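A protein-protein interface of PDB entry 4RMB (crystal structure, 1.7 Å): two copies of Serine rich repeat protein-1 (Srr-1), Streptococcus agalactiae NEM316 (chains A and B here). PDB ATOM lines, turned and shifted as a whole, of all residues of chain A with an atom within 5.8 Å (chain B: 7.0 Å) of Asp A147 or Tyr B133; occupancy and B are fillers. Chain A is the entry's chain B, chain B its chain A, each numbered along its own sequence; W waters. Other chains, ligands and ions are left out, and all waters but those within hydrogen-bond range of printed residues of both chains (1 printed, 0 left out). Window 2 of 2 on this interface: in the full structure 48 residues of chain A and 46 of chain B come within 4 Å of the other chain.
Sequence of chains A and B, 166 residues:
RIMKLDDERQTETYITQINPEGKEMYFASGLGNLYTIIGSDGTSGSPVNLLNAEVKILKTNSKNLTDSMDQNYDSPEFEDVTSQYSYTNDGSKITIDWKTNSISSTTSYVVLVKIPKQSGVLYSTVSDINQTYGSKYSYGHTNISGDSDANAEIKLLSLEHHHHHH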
ATOM      1  N   ASN A 143      -5.972  -8.710   4.292  1.00  0.00           N
ATOM      2  CA  ASN A 143      -4.928  -9.275   5.150  1.00  0.00           C
ATOM      3  C   ASN A 143      -5.596  -9.312   6.517  1.00  0.00           C
ATOM      4  O   ASN A 143      -5.924  -8.271   7.074  1.00  0.00           O
ATOM      5  CB  ASN A 143      -3.725  -8.334   5.180  1.00  0.00           C
ATOM      6  CG  ASN A 143      -2.593  -8.856   6.042  1.00  0.00           C
ATOM      7  OD1 ASN A 143      -2.820  -9.494   7.064  1.00  0.00           O
ATOM      8  ND2 ASN A 143      -1.361  -8.561   5.640  1.00  0.00           N
ATOM      9  N   ILE A 144      -5.792 -10.507   7.063  1.00  0.00           N
ATOM     10  CA  ILE A 144      -6.486 -10.636   8.333  1.00  0.00           C
ATOM     11  C   ILE A 144      -5.875  -9.892   9.518  1.00  0.00           C
ATOM     12  O   ILE A 144      -6.576  -9.150  10.205  1.00  0.00           O
ATOM     13  CB  ILE A 144      -6.680 -12.127   8.696  1.00  0.00           C
ATOM     14  CG1 ILE A 144      -7.425 -12.834   7.552  1.00  0.00           C
ATOM     15  CG2 ILE A 144      -7.471 -12.252   9.998  1.00  0.00           C
ATOM     16  CD1 ILE A 144      -7.602 -14.342   7.741  1.00  0.00           C
ATOM     17  N   SER A 145      -4.581 -10.075   9.757  1.00  0.00           N
ATOM     18  CA  SER A 145      -3.922  -9.414  10.885  1.00  0.00           C
ATOM     19  C   SER A 145      -3.475  -7.993  10.572  1.00  0.00           C
ATOM     20  O   SER A 145      -3.358  -7.156  11.474  1.00  0.00           O
ATOM     21  CB  SER A 145      -2.700 -10.221  11.333  1.00  0.00           C
ATOM     22  OG  SER A 145      -1.630 -10.076  10.411  1.00  0.00           O
ATOM     23  N   GLY A 146      -3.226  -7.724   9.296  1.00  0.00           N
ATOM     24  CA  GLY A 146      -2.764  -6.410   8.899  1.00  0.00           C
ATOM     25  C   GLY A 146      -1.254  -6.313   9.033  1.00  0.00           C
ATOM     26  O   GLY A 146      -0.684  -5.239   8.870  1.00  0.00           O
ATOM     27  N   ASP A 147      -0.595  -7.432   9.328  1.00  0.00           N
ATOM     28  CA  ASP A 147       0.858  -7.418   9.470  1.00  0.00           C
ATOM     29  C   ASP A 147       1.532  -7.311   8.111  1.00  0.00           C
ATOM     30  O   ASP A 147       1.094  -7.928   7.140  1.00  0.00           O
ATOM     31  CB  ASP A 147       1.363  -8.688  10.165  1.00  0.00           C
ATOM     32  CG  ASP A 147       0.844  -8.830  11.583  1.00  0.00           C
ATOM     33  OD1 ASP A 147       0.481  -7.805  12.197  1.00  0.00           O
ATOM     34  OD2 ASP A 147       0.815  -9.971  12.090  1.00  0.00           O
ATOM     35  N   SER A 148       2.600  -6.526   8.046  1.00  0.00           N
ATOM     36  CA  SER A 148       3.352  -6.361   6.810  1.00  0.00           C
ATOM     37  C   SER A 148       4.550  -7.302   6.833  1.00  0.00           C
ATOM     38  O   SER A 148       5.670  -6.889   7.136  1.00  0.00           O
ATOM     39  CB  SER A 148       3.833  -4.915   6.665  1.00  0.00           C
ATOM     40  OG  SER A 148       2.737  -4.023   6.556  1.00  0.00           O
ATOM     41  N   ASP A 149       4.309  -8.570   6.523  1.00  0.00           N
ATOM     42  CA  ASP A 149       5.372  -9.567   6.507  1.00  0.00           C
ATOM     43  C   ASP A 149       5.461 -10.276   5.156  1.00  0.00           C
ATOM     44  O   ASP A 149       4.849  -9.844   4.174  1.00  0.00           O
ATOM     45  CB  ASP A 149       5.160 -10.597   7.624  1.00  0.00           C
ATOM     46  CG  ASP A 149       3.766 -11.195   7.612  1.00  0.00           C
ATOM     47  OD1 ASP A 149       3.116 -11.171   6.545  1.00  0.00           O
ATOM     48  OD2 ASP A 149       3.325 -11.698   8.669  1.00  0.00           O
ATOM     49  N   ASN A 151       4.196 -13.113   4.128  1.00  0.00           N
ATOM     50  CA  ASN A 151       2.917 -13.609   3.631  1.00  0.00           C
ATOM     51  C   ASN A 151       2.017 -12.526   3.045  1.00  0.00           C
ATOM     52  O   ASN A 151       1.188 -12.810   2.179  1.00  0.00           O
ATOM     53  CB  ASN A 151       2.179 -14.374   4.733  1.00  0.00           C
ATOM     54  CG  ASN A 151       2.874 -15.669   5.093  1.00  0.00           C
ATOM     55  OD1 ASN A 151       3.353 -16.384   4.212  1.00  0.00           O
ATOM     56  ND2 ASN A 151       2.930 -15.984   6.383  1.00  0.00           N
ATOM     57  N   ALA A 152       2.184 -11.292   3.504  1.00  0.00           N
ATOM     58  CA  ALA A 152       1.381 -10.184   3.002  1.00  0.00           C
ATOM     59  C   ALA A 152       1.840  -9.770   1.604  1.00  0.00           C
ATOM     60  O   ALA A 152       1.150  -9.022   0.912  1.00  0.00           O
ATOM     61  CB  ALA A 152       1.481  -8.994   3.952  1.00  0.00           C
ATOM     62  N   TYR B  26       4.828 -19.696   4.926  1.00  0.00           N
ATOM     63  CA  TYR B  26       5.208 -20.138   6.260  1.00  0.00           C
ATOM     64  C   TYR B  26       4.538 -19.344   7.377  1.00  0.00           C
ATOM     65  O   TYR B  26       4.489 -18.119   7.336  1.00  0.00           O
ATOM     66  CB  TYR B  26       6.730 -20.034   6.401  1.00  0.00           C
ATOM     67  CG  TYR B  26       7.258 -20.351   7.778  1.00  0.00           C
ATOM     68  CD1 TYR B  26       7.183 -21.642   8.295  1.00  0.00           C
ATOM     69  CD2 TYR B  26       7.836 -19.356   8.568  1.00  0.00           C
ATOM     70  CE1 TYR B  26       7.670 -21.941   9.567  1.00  0.00           C
ATOM     71  CE2 TYR B  26       8.328 -19.642   9.842  1.00  0.00           C
ATOM     72  CZ  TYR B  26       8.240 -20.936  10.335  1.00  0.00           C
ATOM     73  OH  TYR B  26       8.719 -21.225  11.594  1.00  0.00           O
ATOM     74  N   PHE B  27       4.023 -20.057   8.372  1.00  0.00           N
ATOM     75  CA  PHE B  27       3.390 -19.429   9.527  1.00  0.00           C
ATOM     76  C   PHE B  27       4.410 -19.426  10.655  1.00  0.00           C
ATOM     77  O   PHE B  27       4.911 -20.482  11.048  1.00  0.00           O
ATOM     78  CB  PHE B  27       2.153 -20.219   9.966  1.00  0.00           C
ATOM     79  CG  PHE B  27       0.856 -19.708   9.393  1.00  0.00           C
ATOM     80  CD1 PHE B  27       0.838 -18.944   8.230  1.00  0.00           C
ATOM     81  CD2 PHE B  27      -0.355 -20.033  10.002  1.00  0.00           C
ATOM     82  CE1 PHE B  27      -0.373 -18.512   7.678  1.00  0.00           C
ATOM     83  CE2 PHE B  27      -1.568 -19.610   9.461  1.00  0.00           C
ATOM     84  CZ  PHE B  27      -1.576 -18.845   8.295  1.00  0.00           C
ATOM     85  N   ALA B  28       4.718 -18.238  11.165  1.00  0.00           N
ATOM     86  CA  ALA B  28       5.680 -18.096  12.250  1.00  0.00           C
ATOM     87  C   ALA B  28       5.322 -19.019  13.402  1.00  0.00           C
ATOM     88  O   ALA B  28       4.153 -19.325  13.627  1.00  0.00           O
ATOM     89  CB  ALA B  28       5.708 -16.653  12.734  1.00  0.00           C
ATOM     90  N   LEU B  31       1.879 -19.606  15.804  1.00  0.00           N
ATOM     91  CA  LEU B  31       0.639 -19.449  15.056  1.00  0.00           C
ATOM     92  C   LEU B  31      -0.088 -20.774  14.856  1.00  0.00           C
ATOM     93  O   LEU B  31      -1.304 -20.796  14.661  1.00  0.00           O
ATOM     94  CB  LEU B  31       0.929 -18.835  13.682  1.00  0.00           C
ATOM     95  N   THR B 125     -10.258 -18.801   3.520  1.00  0.00           N
ATOM     96  CA  THR B 125      -9.030 -18.263   4.084  1.00  0.00           C
ATOM     97  C   THR B 125      -7.870 -19.239   4.032  1.00  0.00           C
ATOM     98  O   THR B 125      -8.016 -20.416   3.693  1.00  0.00           O
ATOM     99  CB  THR B 125      -9.163 -17.963   5.595  1.00  0.00           C
ATOM    100  OG1 THR B 125      -9.136 -19.202   6.325  1.00  0.00           O
ATOM    101  CG2 THR B 125     -10.448 -17.230   5.905  1.00  0.00           C
ATOM    102  N   VAL B 126      -6.710 -18.680   4.353  1.00  0.00           N
ATOM    103  CA  VAL B 126      -5.488 -19.423   4.592  1.00  0.00           C
ATOM    104  C   VAL B 126      -5.175 -18.630   5.852  1.00  0.00           C
ATOM    105  O   VAL B 126      -4.780 -17.461   5.791  1.00  0.00           O
ATOM    106  CB  VAL B 126      -4.387 -19.226   3.553  1.00  0.00           C
ATOM    107  CG1 VAL B 126      -3.071 -19.758   4.121  1.00  0.00           C
ATOM    108  CG2 VAL B 126      -4.728 -20.006   2.290  1.00  0.00           C
ATOM    109  N   SER B 127      -5.412 -19.258   6.999  1.00  0.00           N
ATOM    110  CA  SER B 127      -5.229 -18.587   8.274  1.00  0.00           C
ATOM    111  C   SER B 127      -5.021 -19.567   9.414  1.00  0.00           C
ATOM    112  O   SER B 127      -4.965 -20.778   9.215  1.00  0.00           O
ATOM    113  CB  SER B 127      -6.476 -17.766   8.586  1.00  0.00           C
ATOM    114  OG  SER B 127      -7.618 -18.613   8.719  1.00  0.00           O
ATOM    115  N   ASP B 128      -4.899 -19.014  10.616  1.00  0.00           N
ATOM    116  CA  ASP B 128      -4.775 -19.831  11.806  1.00  0.00           C
ATOM    117  C   ASP B 128      -6.221 -20.251  12.056  1.00  0.00           C
ATOM    118  O   ASP B 128      -7.145 -19.696  11.447  1.00  0.00           O
ATOM    119  CB  ASP B 128      -4.234 -19.003  12.979  1.00  0.00           C
ATOM    120  CG  ASP B 128      -5.136 -17.842  13.344  1.00  0.00           C
ATOM    121  OD1 ASP B 128      -5.506 -17.067  12.439  1.00  0.00           O
ATOM    122  OD2 ASP B 128      -5.469 -17.693  14.541  1.00  0.00           O
ATOM    123  N   ILE B 129      -6.428 -21.218  12.938  1.00  0.00           N
ATOM    124  CA  ILE B 129      -7.776 -21.702  13.207  1.00  0.00           C
ATOM    125  C   ILE B 129      -8.731 -20.622  13.713  1.00  0.00           C
ATOM    126  O   ILE B 129      -9.931 -20.684  13.453  1.00  0.00           O
ATOM    127  CB  ILE B 129      -7.751 -22.876  14.218  1.00  0.00           C
ATOM    128  CG1 ILE B 129      -9.052 -23.671  14.124  1.00  0.00           C
ATOM    129  CG2 ILE B 129      -7.569 -22.347  15.632  1.00  0.00           C
ATOM    130  CD1 ILE B 129      -9.070 -24.915  14.992  1.00  0.00           C
ATOM    131  N   ASN B 130      -8.200 -19.628  14.420  1.00  0.00           N
ATOM    132  CA  ASN B 130      -9.034 -18.560  14.970  1.00  0.00           C
ATOM    133  C   ASN B 130      -9.225 -17.349  14.058  1.00  0.00           C
ATOM    134  O   ASN B 130      -9.840 -16.359  14.457  1.00  0.00           O
ATOM    135  CB  ASN B 130      -8.463 -18.092  16.312  1.00  0.00           C
ATOM    136  CG  ASN B 130      -8.364 -19.214  17.324  1.00  0.00           C
ATOM    137  OD1 ASN B 130      -9.345 -19.901  17.598  1.00  0.00           O
ATOM    138  ND2 ASN B 130      -7.175 -19.403  17.888  1.00  0.00           N
ATOM    139  N   GLN B 131      -8.708 -17.424  12.835  1.00  0.00           N
ATOM    140  CA  GLN B 131      -8.844 -16.321  11.888  1.00  0.00           C
ATOM    141  C   GLN B 131      -8.344 -14.981  12.423  1.00  0.00           C
ATOM    142  O   GLN B 131      -9.043 -13.974  12.331  1.00  0.00           O
ATOM    143  CB  GLN B 131     -10.302 -16.163  11.449  1.00  0.00           C
ATOM    144  CG  GLN B 131     -10.811 -17.268  10.552  1.00  0.00           C
ATOM    145  CD  GLN B 131     -12.196 -16.975  10.007  1.00  0.00           C
ATOM    146  OE1 GLN B 131     -12.401 -15.988   9.295  1.00  0.00           O
ATOM    147  NE2 GLN B 131     -13.154 -17.829  10.338  1.00  0.00           N
ATOM    148  N   THR B 132      -7.137 -14.970  12.977  1.00  0.00           N
ATOM    149  CA  THR B 132      -6.557 -13.736  13.492  1.00  0.00           C
ATOM    150  C   THR B 132      -5.328 -13.376  12.663  1.00  0.00           C
ATOM    151  O   THR B 132      -4.755 -12.297  12.818  1.00  0.00           O
ATOM    152  CB  THR B 132      -6.130 -13.879  14.971  1.00  0.00           C
ATOM    153  OG1 THR B 132      -5.062 -14.826  15.077  1.00  0.00           O
ATOM    154  CG2 THR B 132      -7.301 -14.342  15.821  1.00  0.00           C
ATOM    155  N   TYR B 133      -4.934 -14.284  11.776  1.00  0.00           N
ATOM    156  CA  TYR B 133      -3.765 -14.078  10.924  1.00  0.00           C
ATOM    157  C   TYR B 133      -3.962 -14.787   9.588  1.00  0.00           C
ATOM    158  O   TYR B 133      -4.564 -15.859   9.535  1.00  0.00           O
ATOM    159  CB  TYR B 133      -2.509 -14.648  11.595  1.00  0.00           C
ATOM    160  CG  TYR B 133      -1.245 -14.478  10.774  1.00  0.00           C
ATOM    161  CD1 TYR B 133      -0.486 -13.310  10.859  1.00  0.00           C
ATOM    162  CD2 TYR B 133      -0.830 -15.469   9.885  1.00  0.00           C
ATOM    163  CE1 TYR B 133       0.650 -13.131  10.081  1.00  0.00           C
ATOM    164  CE2 TYR B 133       0.310 -15.297   9.095  1.00  0.00           C
ATOM    165  CZ  TYR B 133       1.043 -14.126   9.199  1.00  0.00           C
ATOM    166  OH  TYR B 133       2.165 -13.946   8.428  1.00  0.00           O
ATOM    167  N   GLY B 134      -3.455 -14.186   8.516  1.00  0.00           N
ATOM    168  CA  GLY B 134      -3.565 -14.811   7.214  1.00  0.00           C
ATOM    169  C   GLY B 134      -4.233 -13.959   6.156  1.00  0.00           C
ATOM    170  O   GLY B 134      -4.147 -12.731   6.174  1.00  0.00           O
ATOM    171  N   SER B 135      -4.908 -14.621   5.228  1.00  0.00           N
ATOM    172  CA  SER B 135      -5.579 -13.925   4.140  1.00  0.00           C
ATOM    173  C   SER B 135      -6.998 -14.458   3.970  1.00  0.00           C
ATOM    174  O   SER B 135      -7.231 -15.656   4.077  1.00  0.00           O
ATOM    175  CB  SER B 135      -4.788 -14.119   2.843  1.00  0.00           C
ATOM    176  OG  SER B 135      -5.382 -13.400   1.774  1.00  0.00           O
HETATM  177  O   HOH W   1      -2.062 -11.617   8.319  1.00  0.00           O
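Water W1 lies within hydrogen-bond range of the side-chain amide oxygen of Asn A143 (2.6 Å), the side-chain hydroxyl of Ser A145 (2.6 Å) and the backbone NH of Gly B134 (2.9 Å).
Asp A147 touches one residue of chain B. Of chain A, only Ile A144 (3.7 Å), Ser A145 (3.5 Å), Asp A147 (3.7 Å), Asp A149 (2.5 Å) and Asn A151 (3.0 Å) come within 4 Å of Tyr B133. No residue of chain B comes within 4 Å of Gly A146. Of the printed residues of chain A, Gln B131 touches Ile A144 (3.3 Å). Of the printed residues of chain B, Asn A151 touches Tyr B26 and Tyr B133. Printed residues of chain B within 4 Å of Ile A144: Ser B127 (3.7 Å), Gln B131 (3.3 Å), Thr B132 (3.6 Å), Tyr B133 (3.7 Å), Gly B134 (2.9 Å) and Ser B135 (3.7 Å). Printed residues of chain A within 4 Å of Gly B134: Asn A143 (3.6 Å) and Ile A144 (2.9 Å). The nearest printed residue of chain B that does not touch Asn A143 is Ser B135 (4.8 Å).
O of Gly B134 touches OD1 of Asn A143, at 3.6 Å. CB of Ser B127 touches CD1 of Ile A144, 3.7 Å away. Gln B131 touches Ile A144 (O to CG2, 3.3 Å). Ile A144 touches Thr B132. Ile A144 touches Tyr B133. Ile A144 touches Ser B135 (CD1 to N, 3.7 Å). O of Thr B132 touches CB of Ser A145, at 3.3 Å. CD1 of Tyr B133 touches OG of Ser A145, 3.5 Å away. Tyr B133 touches Asp A147 (CE1 to OD2, 3.7 Å).
OH of Tyr B133 sits at hydrogen-bond distance from OD2 of Asp A149 (2.5 Å). The backbone carbonyl oxygen (O) of Tyr B26 sits at hydrogen-bond distance from the side-chain amide nitrogen (ND2) of Asn A151, at 2.8 Å. The backbone carbonyl oxygen (O) of Gly B134 is in hydrogen-bond range of the backbone NH (N) of Ile A144 (2.9 Å). The side-chain hydroxyl (OH) of Tyr B133 lies within hydrogen-bond range of the side-chain amide nitrogen (ND2) of Asn A151 (3.0 Å).
The side-chain amide nitrogen of Asn A143 sits at hydrogen-bond distance from the backbone carbonyl oxygen of Asp A147, at 2.9 Å. OG1 of Thr B125 is in hydrogen-bond range of OG of Ser B127, at 2.9 Å. The side-chain carboxylate of Asp A149 sits close to the backbone NH of Asn A151 (3.3 Å). N of Ser B135 is in hydrogen-bond range of O of Val B126, 2.9 Å away. OD1 of Asp B128 lies within hydrogen-bond range of N of Thr B132. The backbone NH of Tyr B133 lies within hydrogen-bond range of the side-chain carboxylate of Asp B128.
No position is printed for both chains.
Of the 9 printed residues of chain A, 6 touch a printed residue of chain B. Hydrophobic or aromatic side chains of chain A within 4 Å of the printed part of chain B: Ile A144. Among the printed residues, no Asp or Glu carboxylate lies within 4 Å of a Lys or Arg side-chain nitrogen of the other chain.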
